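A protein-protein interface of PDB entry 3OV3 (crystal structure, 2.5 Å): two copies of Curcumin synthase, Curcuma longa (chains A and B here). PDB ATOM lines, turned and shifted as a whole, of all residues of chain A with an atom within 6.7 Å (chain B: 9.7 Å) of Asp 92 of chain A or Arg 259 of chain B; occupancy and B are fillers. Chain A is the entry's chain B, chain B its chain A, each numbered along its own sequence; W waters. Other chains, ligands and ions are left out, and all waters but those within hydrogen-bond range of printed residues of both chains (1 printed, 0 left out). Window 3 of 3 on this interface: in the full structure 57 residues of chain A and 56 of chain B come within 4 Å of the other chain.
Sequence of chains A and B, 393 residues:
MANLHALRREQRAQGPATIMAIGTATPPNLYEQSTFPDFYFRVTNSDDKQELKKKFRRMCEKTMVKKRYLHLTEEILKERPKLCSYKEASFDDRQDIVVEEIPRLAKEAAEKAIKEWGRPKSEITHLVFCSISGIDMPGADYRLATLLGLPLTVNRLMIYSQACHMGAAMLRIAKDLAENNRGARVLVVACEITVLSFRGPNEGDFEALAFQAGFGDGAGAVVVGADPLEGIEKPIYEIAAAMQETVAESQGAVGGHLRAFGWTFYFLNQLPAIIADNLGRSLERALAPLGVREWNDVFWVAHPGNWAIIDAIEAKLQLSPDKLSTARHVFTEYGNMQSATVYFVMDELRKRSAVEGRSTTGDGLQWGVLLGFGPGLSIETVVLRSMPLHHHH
The backbone carbonyl oxygen (O) of Ala 260 of chain A is in hydrogen-bond range of the backbone NH (N) of Phe 91 of chain A.
The backbone NH (N) of Phe 91 of chain B lies within hydrogen-bond range of the backbone carbonyl oxygen (O) of Ala 260 of chain B.
OD2 of Asp 96 of chain A lies within salt-bridge range of NH1 of Arg 80 of chain A, 3.2 Å away.
The backbone NH (N) of Ser 90 of chain A sits at hydrogen-bond distance from the backbone carbonyl oxygen (O) of Ala 260 of chain A (2.9 Å).
Hydrophobic or aromatic side chains of chain B that line the printed part of chain A: Phe 91, His 257, Leu 258 and Ala 260.
Of the 13 printed residues of chain A, 6 touch a printed residue of chain B.
Printed residues of chain A that touch a printed residue of chain B: Phe 91, Asp 92, Gln 95, Asp 96, Asp 136 and Ala 260.
Among the printed residues, 13 pairs touch across the chains.
Water W1 bridges OD1 of Asp 136 of chain A (2.7 Å) and N of Leu 258 of chain B (2.9 Å).
Of chain B, only Arg 259 (3.3 Å) and Ala 260 (2.8 Å) come within 4 Å of Asp 92 of chain A.
Printed residues of chain B within 4 Å of Asp 96 of chain A: Arg 259.
Of the printed residues of chain B, Ala 260 of chain A touches Phe 91 and Asp 92.
Of the printed residues of chain A, His 257 of chain B touches Asp 136 (2.6 Å).
Of the printed residues of chain A, Leu 258 of chain B touches Phe 91 (3.9 Å) and Gln 95 (2.9 Å).
Of chain A, only Phe 91, Asp 92, Gln 95 and Asp 96 come within 4 Å of Arg 259 of chain B.
The nearest printed residue of chain B that does not touch Gln 95 of chain A is His 257 of chain B (5.9 Å).
Among the printed residues, pairs that only touch across the chains: Phe 91 of chain A with Phe 91 of chain B (3.9 Å), Phe 91 of chain A with Leu 258 of chain B (3.9 Å), Phe 91 of chain A with Arg 259 of chain B (3.6 Å), Phe 91 of chain A with Ala 260 of chain B (3.7 Å), Gln 95 of chain A with Arg 259 of chain B (3.7 Å) and Ala 260 of chain A with Phe 91 of chain B (3.8 Å).
The backbone NH (N) of Ala 260 of chain B sits at hydrogen-bond distance from the side-chain carboxylate (OD1) of Asp 92 of chain A.
OD1 of Asp 136 of chain A lies close to O of Gly 256 of chain B (3.1 Å).
The guanidinium group (NH1) of Arg 259 of chain B lies within salt-bridge range of the side-chain carboxylate (OD1) of Asp 96 of chain A.
The guanidinium group (NE) of Arg 259 of chain B lies within salt-bridge range of the side-chain carboxylate (OD1) of Asp 92 of chain A (3.6 Å).
The backbone carbonyl oxygen of Leu 258 of chain B is in hydrogen-bond range of the side-chain amide nitrogen of Gln 95 of chain A (2.9 Å).
N of Ala 260 of chain A lies within hydrogen-bond range of OD1 of Asp 92 of chain B, 2.8 Å away.
The side-chain carboxylate (OD1) of Asp 136 of chain A lies within hydrogen-bond range of a ring nitrogen (ND1) of His 257 of chain B (2.6 Å).
Phe 91 of chain A touches its own counterpart, Phe 91 of chain B.
Phe 91 of chain A touches Ala 260 of chain B, and with the chains exchanged Ala 260 of chain A touches Phe 91 of chain B.
Asp 92 of chain A touches Ala 260 of chain B, and with the chains exchanged Ala 260 of chain A touches Asp 92 of chain B.
Positions printed for both chains: 89, 90, 91, 92, 94, 95 and 260.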
ATOM      1  N   ARG A  80       0.989   9.303  38.852  1.00  0.00           N
ATOM      2  CA  ARG A  80       1.821   8.289  38.214  1.00  0.00           C
ATOM      3  C   ARG A  80       1.639   6.894  38.843  1.00  0.00           C
ATOM      4  O   ARG A  80       2.572   6.352  39.428  1.00  0.00           O
ATOM      5  CB  ARG A  80       3.293   8.735  38.244  1.00  0.00           C
ATOM      6  CG  ARG A  80       3.563  10.022  37.454  1.00  0.00           C
ATOM      7  CD  ARG A  80       4.903  10.637  37.815  1.00  0.00           C
ATOM      8  NE  ARG A  80       5.155  11.954  37.205  1.00  0.00           N
ATOM      9  CZ  ARG A  80       5.666  12.164  35.986  1.00  0.00           C
ATOM     10  NH1 ARG A  80       5.977  11.150  35.180  1.00  0.00           N
ATOM     11  NH2 ARG A  80       5.851  13.401  35.560  1.00  0.00           N
ATOM     12  N   ALA A  89       6.516  -2.499  34.186  1.00  0.00           N
ATOM     13  CA  ALA A  89       7.385  -1.449  33.659  1.00  0.00           C
ATOM     14  C   ALA A  89       6.932  -0.083  34.193  1.00  0.00           C
ATOM     15  O   ALA A  89       5.751   0.284  34.104  1.00  0.00           O
ATOM     16  CB  ALA A  89       7.435  -1.467  32.120  1.00  0.00           C
ATOM     17  N   SER A  90       7.876   0.638  34.784  1.00  0.00           N
ATOM     18  CA  SER A  90       7.590   1.915  35.408  1.00  0.00           C
ATOM     19  C   SER A  90       8.743   2.888  35.213  1.00  0.00           C
ATOM     20  O   SER A  90       8.760   3.966  35.796  1.00  0.00           O
ATOM     21  CB  SER A  90       7.366   1.691  36.903  1.00  0.00           C
ATOM     22  OG  SER A  90       8.386   0.857  37.420  1.00  0.00           O
ATOM     23  N   PHE A  91       9.718   2.489  34.403  1.00  0.00           N
ATOM     24  CA  PHE A  91      10.982   3.198  34.308  1.00  0.00           C
ATOM     25  C   PHE A  91      10.839   4.669  33.877  1.00  0.00           C
ATOM     26  O   PHE A  91      11.477   5.556  34.445  1.00  0.00           O
ATOM     27  CB  PHE A  91      11.923   2.438  33.369  1.00  0.00           C
ATOM     28  CG  PHE A  91      13.353   2.848  33.481  1.00  0.00           C
ATOM     29  CD1 PHE A  91      13.938   3.073  34.714  1.00  0.00           C
ATOM     30  CD2 PHE A  91      14.131   2.988  32.352  1.00  0.00           C
ATOM     31  CE1 PHE A  91      15.276   3.440  34.798  1.00  0.00           C
ATOM     32  CE2 PHE A  91      15.462   3.354  32.444  1.00  0.00           C
ATOM     33  CZ  PHE A  91      16.031   3.564  33.662  1.00  0.00           C
ATOM     34  N   ASP A  92       9.986   4.906  32.887  1.00  0.00           N
ATOM     35  CA  ASP A  92       9.809   6.234  32.311  1.00  0.00           C
ATOM     36  C   ASP A  92       9.361   7.216  33.374  1.00  0.00           C
ATOM     37  O   ASP A  92       9.967   8.288  33.510  1.00  0.00           O
ATOM     38  CB  ASP A  92       8.859   6.217  31.089  1.00  0.00           C
ATOM     39  CG  ASP A  92       9.327   5.250  30.003  1.00  0.00           C
ATOM     40  OD1 ASP A  92      10.556   5.167  29.757  1.00  0.00           O
ATOM     41  OD2 ASP A  92       8.476   4.538  29.421  1.00  0.00           O
ATOM     42  N   ASP A  93       8.315   6.848  34.117  1.00  0.00           N
ATOM     43  CA  ASP A  93       7.801   7.676  35.199  1.00  0.00           C
ATOM     44  C   ASP A  93       8.919   7.972  36.212  1.00  0.00           C
ATOM     45  O   ASP A  93       9.133   9.120  36.612  1.00  0.00           O
ATOM     46  CB  ASP A  93       6.574   7.010  35.880  1.00  0.00           C
ATOM     47  CG  ASP A  93       5.307   7.036  35.001  1.00  0.00           C
ATOM     48  OD1 ASP A  93       4.903   5.975  34.469  1.00  0.00           O
ATOM     49  OD2 ASP A  93       4.714   8.116  34.830  1.00  0.00           O
ATOM     50  N   ARG A  94       9.654   6.943  36.601  1.00  0.00           N
ATOM     51  CA  ARG A  94      10.715   7.101  37.562  1.00  0.00           C
ATOM     52  C   ARG A  94      11.813   8.019  37.045  1.00  0.00           C
ATOM     53  O   ARG A  94      12.380   8.814  37.804  1.00  0.00           O
ATOM     54  CB  ARG A  94      11.292   5.745  37.926  1.00  0.00           C
ATOM     55  CG  ARG A  94      10.278   4.811  38.575  1.00  0.00           C
ATOM     56  CD  ARG A  94      10.866   3.460  38.925  1.00  0.00           C
ATOM     57  NE  ARG A  94       9.817   2.512  39.287  1.00  0.00           N
ATOM     58  CZ  ARG A  94       9.268   2.393  40.497  1.00  0.00           C
ATOM     59  NH1 ARG A  94       9.665   3.168  41.507  1.00  0.00           N
ATOM     60  NH2 ARG A  94       8.320   1.486  40.694  1.00  0.00           N
ATOM     61  N   GLN A  95      12.098   7.922  35.752  1.00  0.00           N
ATOM     62  CA  GLN A  95      13.132   8.730  35.121  1.00  0.00           C
ATOM     63  C   GLN A  95      12.697  10.200  35.013  1.00  0.00           C
ATOM     64  O   GLN A  95      13.481  11.117  35.265  1.00  0.00           O
ATOM     65  CB  GLN A  95      13.516   8.135  33.746  1.00  0.00           C
ATOM     66  CG  GLN A  95      14.500   6.969  33.792  1.00  0.00           C
ATOM     67  CD  GLN A  95      15.923   7.408  34.167  1.00  0.00           C
ATOM     68  OE1 GLN A  95      16.201   7.728  35.321  1.00  0.00           O
ATOM     69  NE2 GLN A  95      16.835   7.418  33.184  1.00  0.00           N
ATOM     70  N   ASP A  96      11.433  10.414  34.662  1.00  0.00           N
ATOM     71  CA  ASP A  96      10.825  11.744  34.642  1.00  0.00           C
ATOM     72  C   ASP A  96      11.066  12.529  35.932  1.00  0.00           C
ATOM     73  O   ASP A  96      11.305  13.745  35.905  1.00  0.00           O
ATOM     74  CB  ASP A  96       9.314  11.636  34.381  1.00  0.00           C
ATOM     75  CG  ASP A  96       8.980  11.401  32.909  1.00  0.00           C
ATOM     76  OD1 ASP A  96       9.914  11.351  32.078  1.00  0.00           O
ATOM     77  OD2 ASP A  96       7.776  11.285  32.579  1.00  0.00           O
ATOM     78  N   ILE A  97      11.005  11.854  37.071  1.00  0.00           N
ATOM     79  CA  ILE A  97      11.210  12.562  38.325  1.00  0.00           C
ATOM     80  C   ILE A  97      12.703  12.735  38.651  1.00  0.00           C
ATOM     81  O   ILE A  97      13.139  13.848  38.972  1.00  0.00           O
ATOM     82  CB  ILE A  97      10.451  11.878  39.456  1.00  0.00           C
ATOM     83  CG1 ILE A  97       8.951  11.859  39.127  1.00  0.00           C
ATOM     84  CG2 ILE A  97      10.762  12.526  40.796  1.00  0.00           C
ATOM     85  CD1 ILE A  97       8.179  10.790  39.884  1.00  0.00           C
ATOM     86  N   VAL A  99      15.509  12.697  36.946  1.00  0.00           N
ATOM     87  CA  VAL A  99      16.344  13.505  36.096  1.00  0.00           C
ATOM     88  C   VAL A  99      16.152  14.961  36.540  1.00  0.00           C
ATOM     89  O   VAL A  99      17.093  15.752  36.629  1.00  0.00           O
ATOM     90  CB  VAL A  99      16.025  13.215  34.626  1.00  0.00           C
ATOM     91  CG1 VAL A  99      16.572  14.315  33.691  1.00  0.00           C
ATOM     92  CG2 VAL A  99      16.622  11.883  34.268  1.00  0.00           C
ATOM     93  N   ASP A 136      20.801  11.077  32.599  1.00  0.00           N
ATOM     94  CA  ASP A 136      20.433  11.737  31.375  1.00  0.00           C
ATOM     95  C   ASP A 136      21.752  12.205  30.735  1.00  0.00           C
ATOM     96  O   ASP A 136      22.801  12.217  31.418  1.00  0.00           O
ATOM     97  CB  ASP A 136      19.559  12.968  31.662  1.00  0.00           C
ATOM     98  CG  ASP A 136      18.694  13.371  30.449  1.00  0.00           C
ATOM     99  OD1 ASP A 136      17.957  12.509  29.889  1.00  0.00           O
ATOM    100  OD2 ASP A 136      18.753  14.549  30.029  1.00  0.00           O
ATOM    101  N   ALA A 260      13.472  -2.664  33.994  1.00  0.00           N
ATOM    102  CA  ALA A 260      12.372  -1.805  33.530  1.00  0.00           C
ATOM    103  C   ALA A 260      11.383  -1.449  34.642  1.00  0.00           C
ATOM    104  O   ALA A 260      10.511  -0.587  34.472  1.00  0.00           O
ATOM    105  CB  ALA A 260      11.662  -2.448  32.410  1.00  0.00           C
ATOM    106  N   TYR B  86      11.305   0.006  17.755  1.00  0.00           N
ATOM    107  CA  TYR B  86      11.928   1.318  17.961  1.00  0.00           C
ATOM    108  C   TYR B  86      11.526   2.091  19.189  1.00  0.00           C
ATOM    109  O   TYR B  86      12.283   2.965  19.618  1.00  0.00           O
ATOM    110  CB  TYR B  86      11.908   2.237  16.732  1.00  0.00           C
ATOM    111  CG  TYR B  86      10.608   2.445  16.043  1.00  0.00           C
ATOM    112  CD1 TYR B  86       9.735   3.453  16.447  1.00  0.00           C
ATOM    113  CD2 TYR B  86      10.275   1.676  14.901  1.00  0.00           C
ATOM    114  CE1 TYR B  86       8.518   3.655  15.759  1.00  0.00           C
ATOM    115  CE2 TYR B  86       9.067   1.869  14.200  1.00  0.00           C
ATOM    116  CZ  TYR B  86       8.199   2.859  14.637  1.00  0.00           C
ATOM    117  OH  TYR B  86       7.016   3.059  13.958  1.00  0.00           O
ATOM    118  N   LYS B  87      10.351   1.806  19.737  1.00  0.00           N
ATOM    119  CA  LYS B  87       9.864   2.547  20.900  1.00  0.00           C
ATOM    120  C   LYS B  87       9.087   1.705  21.946  1.00  0.00           C
ATOM    121  O   LYS B  87       8.654   2.254  22.969  1.00  0.00           O
ATOM    122  CB  LYS B  87       9.063   3.810  20.475  1.00  0.00           C
ATOM    123  CG  LYS B  87       9.853   4.975  19.738  1.00  0.00           C
ATOM    124  CD  LYS B  87      10.976   5.651  20.589  1.00  0.00           C
ATOM    125  CE  LYS B  87      11.699   6.809  19.852  1.00  0.00           C
ATOM    126  NZ  LYS B  87      13.209   6.772  20.018  1.00  0.00           N
ATOM    127  N   GLU B  88       8.920   0.396  21.716  1.00  0.00           N
ATOM    128  CA  GLU B  88       8.447  -0.511  22.783  1.00  0.00           C
ATOM    129  C   GLU B  88       9.512  -0.816  23.845  1.00  0.00           C
ATOM    130  O   GLU B  88      10.720  -0.709  23.580  1.00  0.00           O
ATOM    131  CB  GLU B  88       7.880  -1.817  22.225  1.00  0.00           C
ATOM    132  CG  GLU B  88       6.439  -1.701  21.727  1.00  0.00           C
ATOM    133  CD  GLU B  88       5.398  -1.481  22.851  1.00  0.00           C
ATOM    134  OE1 GLU B  88       5.754  -1.457  24.058  1.00  0.00           O
ATOM    135  OE2 GLU B  88       4.197  -1.343  22.521  1.00  0.00           O
ATOM    136  N   ALA B  89       9.061  -1.196  25.040  1.00  0.00           N
ATOM    137  CA  ALA B  89       9.961  -1.556  26.141  1.00  0.00           C
ATOM    138  C   ALA B  89      10.905  -2.706  25.773  1.00  0.00           C
ATOM    139  O   ALA B  89      10.477  -3.759  25.312  1.00  0.00           O
ATOM    140  CB  ALA B  89       9.159  -1.882  27.414  1.00  0.00           C
ATOM    141  N   SER B  90      12.195  -2.488  25.974  1.00  0.00           N
ATOM    142  CA  SER B  90      13.239  -3.446  25.585  1.00  0.00           C
ATOM    143  C   SER B  90      14.435  -3.363  26.544  1.00  0.00           C
ATOM    144  O   SER B  90      15.449  -4.041  26.344  1.00  0.00           O
ATOM    145  CB  SER B  90      13.701  -3.162  24.151  1.00  0.00           C
ATOM    146  OG  SER B  90      14.154  -1.817  24.006  1.00  0.00           O
ATOM    147  N   PHE B  91      14.319  -2.519  27.570  1.00  0.00           N
ATOM    148  CA  PHE B  91      15.402  -2.281  28.522  1.00  0.00           C
ATOM    149  C   PHE B  91      16.006  -3.549  29.152  1.00  0.00           C
ATOM    150  O   PHE B  91      17.231  -3.675  29.236  1.00  0.00           O
ATOM    151  CB  PHE B  91      14.954  -1.295  29.607  1.00  0.00           C
ATOM    152  CG  PHE B  91      16.075  -0.763  30.458  1.00  0.00           C
ATOM    153  CD1 PHE B  91      17.260  -0.311  29.883  1.00  0.00           C
ATOM    154  CD2 PHE B  91      15.939  -0.698  31.837  1.00  0.00           C
ATOM    155  CE1 PHE B  91      18.299   0.178  30.680  1.00  0.00           C
ATOM    156  CE2 PHE B  91      16.959  -0.207  32.640  1.00  0.00           C
ATOM    157  CZ  PHE B  91      18.148   0.236  32.062  1.00  0.00           C
ATOM    158  N   ASP B  92      15.161  -4.488  29.586  1.00  0.00           N
ATOM    159  CA  ASP B  92      15.681  -5.713  30.209  1.00  0.00           C
ATOM    160  C   ASP B  92      16.549  -6.557  29.279  1.00  0.00           C
ATOM    161  O   ASP B  92      17.584  -7.046  29.708  1.00  0.00           O
ATOM    162  CB  ASP B  92      14.567  -6.566  30.823  1.00  0.00           C
ATOM    163  CG  ASP B  92      13.799  -5.820  31.914  1.00  0.00           C
ATOM    164  OD1 ASP B  92      14.318  -4.782  32.396  1.00  0.00           O
ATOM    165  OD2 ASP B  92      12.677  -6.263  32.278  1.00  0.00           O
ATOM    166  N   ARG B  94      18.293  -5.501  26.736  1.00  0.00           N
ATOM    167  CA  ARG B  94      19.529  -4.734  26.614  1.00  0.00           C
ATOM    168  C   ARG B  94      20.429  -4.875  27.864  1.00  0.00           C
ATOM    169  O   ARG B  94      21.637  -5.148  27.740  1.00  0.00           O
ATOM    170  CB  ARG B  94      19.211  -3.271  26.273  1.00  0.00           C
ATOM    171  CG  ARG B  94      18.329  -3.101  25.019  1.00  0.00           C
ATOM    172  CD  ARG B  94      17.707  -1.716  24.875  1.00  0.00           C
ATOM    173  NE  ARG B  94      16.799  -1.584  23.715  1.00  0.00           N
ATOM    174  CZ  ARG B  94      17.160  -1.445  22.429  1.00  0.00           C
ATOM    175  NH1 ARG B  94      18.446  -1.457  22.031  1.00  0.00           N
ATOM    176  NH2 ARG B  94      16.220  -1.319  21.516  1.00  0.00           N
ATOM    177  N   GLN B  95      19.864  -4.727  29.058  1.00  0.00           N
ATOM    178  CA  GLN B  95      20.659  -4.886  30.293  1.00  0.00           C
ATOM    179  C   GLN B  95      21.336  -6.263  30.418  1.00  0.00           C
ATOM    180  O   GLN B  95      22.517  -6.337  30.765  1.00  0.00           O
ATOM    181  CB  GLN B  95      19.825  -4.622  31.559  1.00  0.00           C
ATOM    182  CG  GLN B  95      19.490  -3.174  31.822  1.00  0.00           C
ATOM    183  CD  GLN B  95      20.727  -2.335  32.124  1.00  0.00           C
ATOM    184  OE1 GLN B  95      21.418  -1.861  31.207  1.00  0.00           O
ATOM    185  NE2 GLN B  95      21.019  -2.155  33.412  1.00  0.00           N
ATOM    186  N   LEU B 196      22.546  -1.034  23.798  1.00  0.00           N
ATOM    187  CA  LEU B 196      21.489  -0.223  24.437  1.00  0.00           C
ATOM    188  C   LEU B 196      20.869   0.847  23.549  1.00  0.00           C
ATOM    189  O   LEU B 196      19.786   1.393  23.886  1.00  0.00           O
ATOM    190  CB  LEU B 196      21.995   0.445  25.722  1.00  0.00           C
ATOM    191  CG  LEU B 196      21.686  -0.202  27.070  1.00  0.00           C
ATOM    192  CD1 LEU B 196      22.682   0.168  28.163  1.00  0.00           C
ATOM    193  CD2 LEU B 196      20.252   0.164  27.463  1.00  0.00           C
ATOM    194  N   SER B 197      21.538   1.184  22.442  1.00  0.00           N
ATOM    195  CA  SER B 197      21.011   2.202  21.500  1.00  0.00           C
ATOM    196  C   SER B 197      20.588   1.658  20.136  1.00  0.00           C
ATOM    197  O   SER B 197      19.915   2.373  19.370  1.00  0.00           O
ATOM    198  CB  SER B 197      21.995   3.375  21.288  1.00  0.00           C
ATOM    199  OG  SER B 197      23.158   2.937  20.582  1.00  0.00           O
ATOM    200  N   ARG B 199      18.437  -0.226  17.404  1.00  0.00           N
ATOM    201  CA  ARG B 199      16.995  -0.423  17.243  1.00  0.00           C
ATOM    202  C   ARG B 199      16.562  -0.311  15.802  1.00  0.00           C
ATOM    203  O   ARG B 199      17.245   0.272  14.996  1.00  0.00           O
ATOM    204  CB  ARG B 199      16.206   0.583  18.095  1.00  0.00           C
ATOM    205  CG  ARG B 199      16.143   1.988  17.488  1.00  0.00           C
ATOM    206  CD  ARG B 199      15.348   2.932  18.363  1.00  0.00           C
ATOM    207  NE  ARG B 199      16.104   3.294  19.553  1.00  0.00           N
ATOM    208  CZ  ARG B 199      15.870   2.786  20.761  1.00  0.00           C
ATOM    209  NH1 ARG B 199      14.882   1.902  20.947  1.00  0.00           N
ATOM    210  NH2 ARG B 199      16.624   3.168  21.794  1.00  0.00           N
ATOM    211  N   GLY B 256      21.223  12.691  25.087  1.00  0.00           N
ATOM    212  CA  GLY B 256      20.306  11.555  25.030  1.00  0.00           C
ATOM    213  C   GLY B 256      19.475  11.334  26.283  1.00  0.00           C
ATOM    214  O   GLY B 256      19.674  12.019  27.308  1.00  0.00           O
ATOM    215  N   HIS B 257      18.558  10.364  26.193  1.00  0.00           N
ATOM    216  CA  HIS B 257      17.729   9.942  27.315  1.00  0.00           C
ATOM    217  C   HIS B 257      17.726   8.439  27.439  1.00  0.00           C
ATOM    218  O   HIS B 257      17.681   7.745  26.422  1.00  0.00           O
ATOM    219  CB  HIS B 257      16.300  10.443  27.139  1.00  0.00           C
ATOM    220  CG  HIS B 257      16.223  11.887  26.775  1.00  0.00           C
ATOM    221  ND1 HIS B 257      16.793  12.874  27.549  1.00  0.00           N
ATOM    222  CD2 HIS B 257      15.693  12.510  25.697  1.00  0.00           C
ATOM    223  CE1 HIS B 257      16.596  14.047  26.974  1.00  0.00           C
ATOM    224  NE2 HIS B 257      15.930  13.854  25.848  1.00  0.00           N
ATOM    225  N   LEU B 258      17.808   7.954  28.678  1.00  0.00           N
ATOM    226  CA  LEU B 258      17.727   6.537  29.015  1.00  0.00           C
ATOM    227  C   LEU B 258      16.319   6.261  29.450  1.00  0.00           C
ATOM    228  O   LEU B 258      15.875   6.741  30.507  1.00  0.00           O
ATOM    229  CB  LEU B 258      18.688   6.176  30.172  1.00  0.00           C
ATOM    230  CG  LEU B 258      18.862   4.674  30.547  1.00  0.00           C
ATOM    231  CD1 LEU B 258      19.071   3.730  29.327  1.00  0.00           C
ATOM    232  CD2 LEU B 258      19.975   4.470  31.564  1.00  0.00           C
ATOM    233  N   ARG B 259      15.596   5.499  28.646  1.00  0.00           N
ATOM    234  CA  ARG B 259      14.172   5.253  28.931  1.00  0.00           C
ATOM    235  C   ARG B 259      13.896   3.767  28.861  1.00  0.00           C
ATOM    236  O   ARG B 259      14.819   2.977  28.671  1.00  0.00           O
ATOM    237  CB  ARG B 259      13.298   6.014  27.920  1.00  0.00           C
ATOM    238  CG  ARG B 259      13.684   7.479  27.706  1.00  0.00           C
ATOM    239  CD  ARG B 259      13.211   8.317  28.869  1.00  0.00           C
ATOM    240  NE  ARG B 259      11.749   8.453  28.902  1.00  0.00           N
ATOM    241  CZ  ARG B 259      11.092   9.087  29.865  1.00  0.00           C
ATOM    242  NH1 ARG B 259      11.770   9.620  30.880  1.00  0.00           N
ATOM    243  NH2 ARG B 259       9.769   9.169  29.837  1.00  0.00           N
ATOM    244  N   ALA B 260      12.629   3.385  28.992  1.00  0.00           N
ATOM    245  CA  ALA B 260      12.247   1.970  28.823  1.00  0.00           C
ATOM    246  C   ALA B 260      12.716   1.324  27.500  1.00  0.00           C
ATOM    247  O   ALA B 260      12.894   0.105  27.440  1.00  0.00           O
ATOM    248  CB  ALA B 260      10.748   1.793  28.990  1.00  0.00           C
ATOM    249  N   PHE B 261      12.916   2.117  26.450  1.00  0.00           N
ATOM    250  CA  PHE B 261      13.294   1.542  25.168  1.00  0.00           C
ATOM    251  C   PHE B 261      14.808   1.496  24.956  1.00  0.00           C
ATOM    252  O   PHE B 261      15.264   1.126  23.871  1.00  0.00           O
ATOM    253  CB  PHE B 261      12.581   2.240  23.981  1.00  0.00           C
ATOM    254  CG  PHE B 261      12.672   3.735  24.010  1.00  0.00           C
ATOM    255  CD1 PHE B 261      13.918   4.380  24.054  1.00  0.00           C
ATOM    256  CD2 PHE B 261      11.501   4.520  23.990  1.00  0.00           C
ATOM    257  CE1 PHE B 261      14.005   5.790  24.094  1.00  0.00           C
ATOM    258  CE2 PHE B 261      11.568   5.937  24.010  1.00  0.00           C
ATOM    259  CZ  PHE B 261      12.821   6.575  24.059  1.00  0.00           C
ATOM    260  N   GLY B 262      15.565   1.866  25.997  1.00  0.00           N
ATOM    261  CA  GLY B 262      17.021   2.002  25.925  1.00  0.00           C
ATOM    262  C   GLY B 262      17.425   3.472  25.780  1.00  0.00           C
ATOM    263  O   GLY B 262      16.683   4.376  26.198  1.00  0.00           O
ATOM    264  N   TRP B 263      18.604   3.699  25.205  1.00  0.00           N
ATOM    265  CA  TRP B 263      19.133   5.031  24.924  1.00  0.00           C
ATOM    266  C   TRP B 263      18.613   5.559  23.583  1.00  0.00           C
ATOM    267  O   TRP B 263      18.613   4.858  22.603  1.00  0.00           O
ATOM    268  CB  TRP B 263      20.673   4.976  24.888  1.00  0.00           C
ATOM    269  CG  TRP B 263      21.303   5.034  26.252  1.00  0.00           C
ATOM    270  CD1 TRP B 263      21.757   3.979  26.979  1.00  0.00           C
ATOM    271  CD2 TRP B 263      21.523   6.209  27.069  1.00  0.00           C
ATOM    272  NE1 TRP B 263      22.269   4.412  28.191  1.00  0.00           N
ATOM    273  CE2 TRP B 263      22.123   5.774  28.277  1.00  0.00           C
ATOM    274  CE3 TRP B 263      21.277   7.580  26.894  1.00  0.00           C
ATOM    275  CZ2 TRP B 263      22.489   6.664  29.312  1.00  0.00           C
ATOM    276  CZ3 TRP B 263      21.651   8.476  27.923  1.00  0.00           C
ATOM    277  CH2 TRP B 263      22.248   8.004  29.112  1.00  0.00           C
ATOM    278  N   THR B 264      18.158   6.799  23.563  1.00  0.00           N
ATOM    279  CA  THR B 264      17.850   7.536  22.326  1.00  0.00           C
ATOM    280  C   THR B 264      18.821   8.712  22.354  1.00  0.00           C
ATOM    281  O   THR B 264      19.035   9.313  23.422  1.00  0.00           O
ATOM    282  CB  THR B 264      16.370   8.020  22.295  1.00  0.00           C
ATOM    283  OG1 THR B 264      16.174   9.037  21.304  1.00  0.00           O
ATOM    284  CG2 THR B 264      15.951   8.599  23.650  1.00  0.00           C
ATOM    285  N   PHE B 265      19.421   9.038  21.209  1.00  0.00           N
ATOM    286  CA  PHE B 265      20.294  10.222  21.119  1.00  0.00           C
ATOM    287  C   PHE B 265      19.739  11.275  20.162  1.00  0.00           C
ATOM    288  O   PHE B 265      18.968  10.951  19.257  1.00  0.00           O
ATOM    289  CB  PHE B 265      21.718   9.837  20.727  1.00  0.00           C
ATOM    290  CG  PHE B 265      22.310   8.761  21.578  1.00  0.00           C
ATOM    291  CD1 PHE B 265      22.569   8.984  22.928  1.00  0.00           C
ATOM    292  CD2 PHE B 265      22.618   7.533  21.034  1.00  0.00           C
ATOM    293  CE1 PHE B 265      23.103   7.976  23.719  1.00  0.00           C
ATOM    294  CE2 PHE B 265      23.181   6.533  21.812  1.00  0.00           C
ATOM    295  CZ  PHE B 265      23.417   6.753  23.155  1.00  0.00           C
HETATM  296  O   HOH W   1      17.158   9.986  30.633  1.00  0.00           O
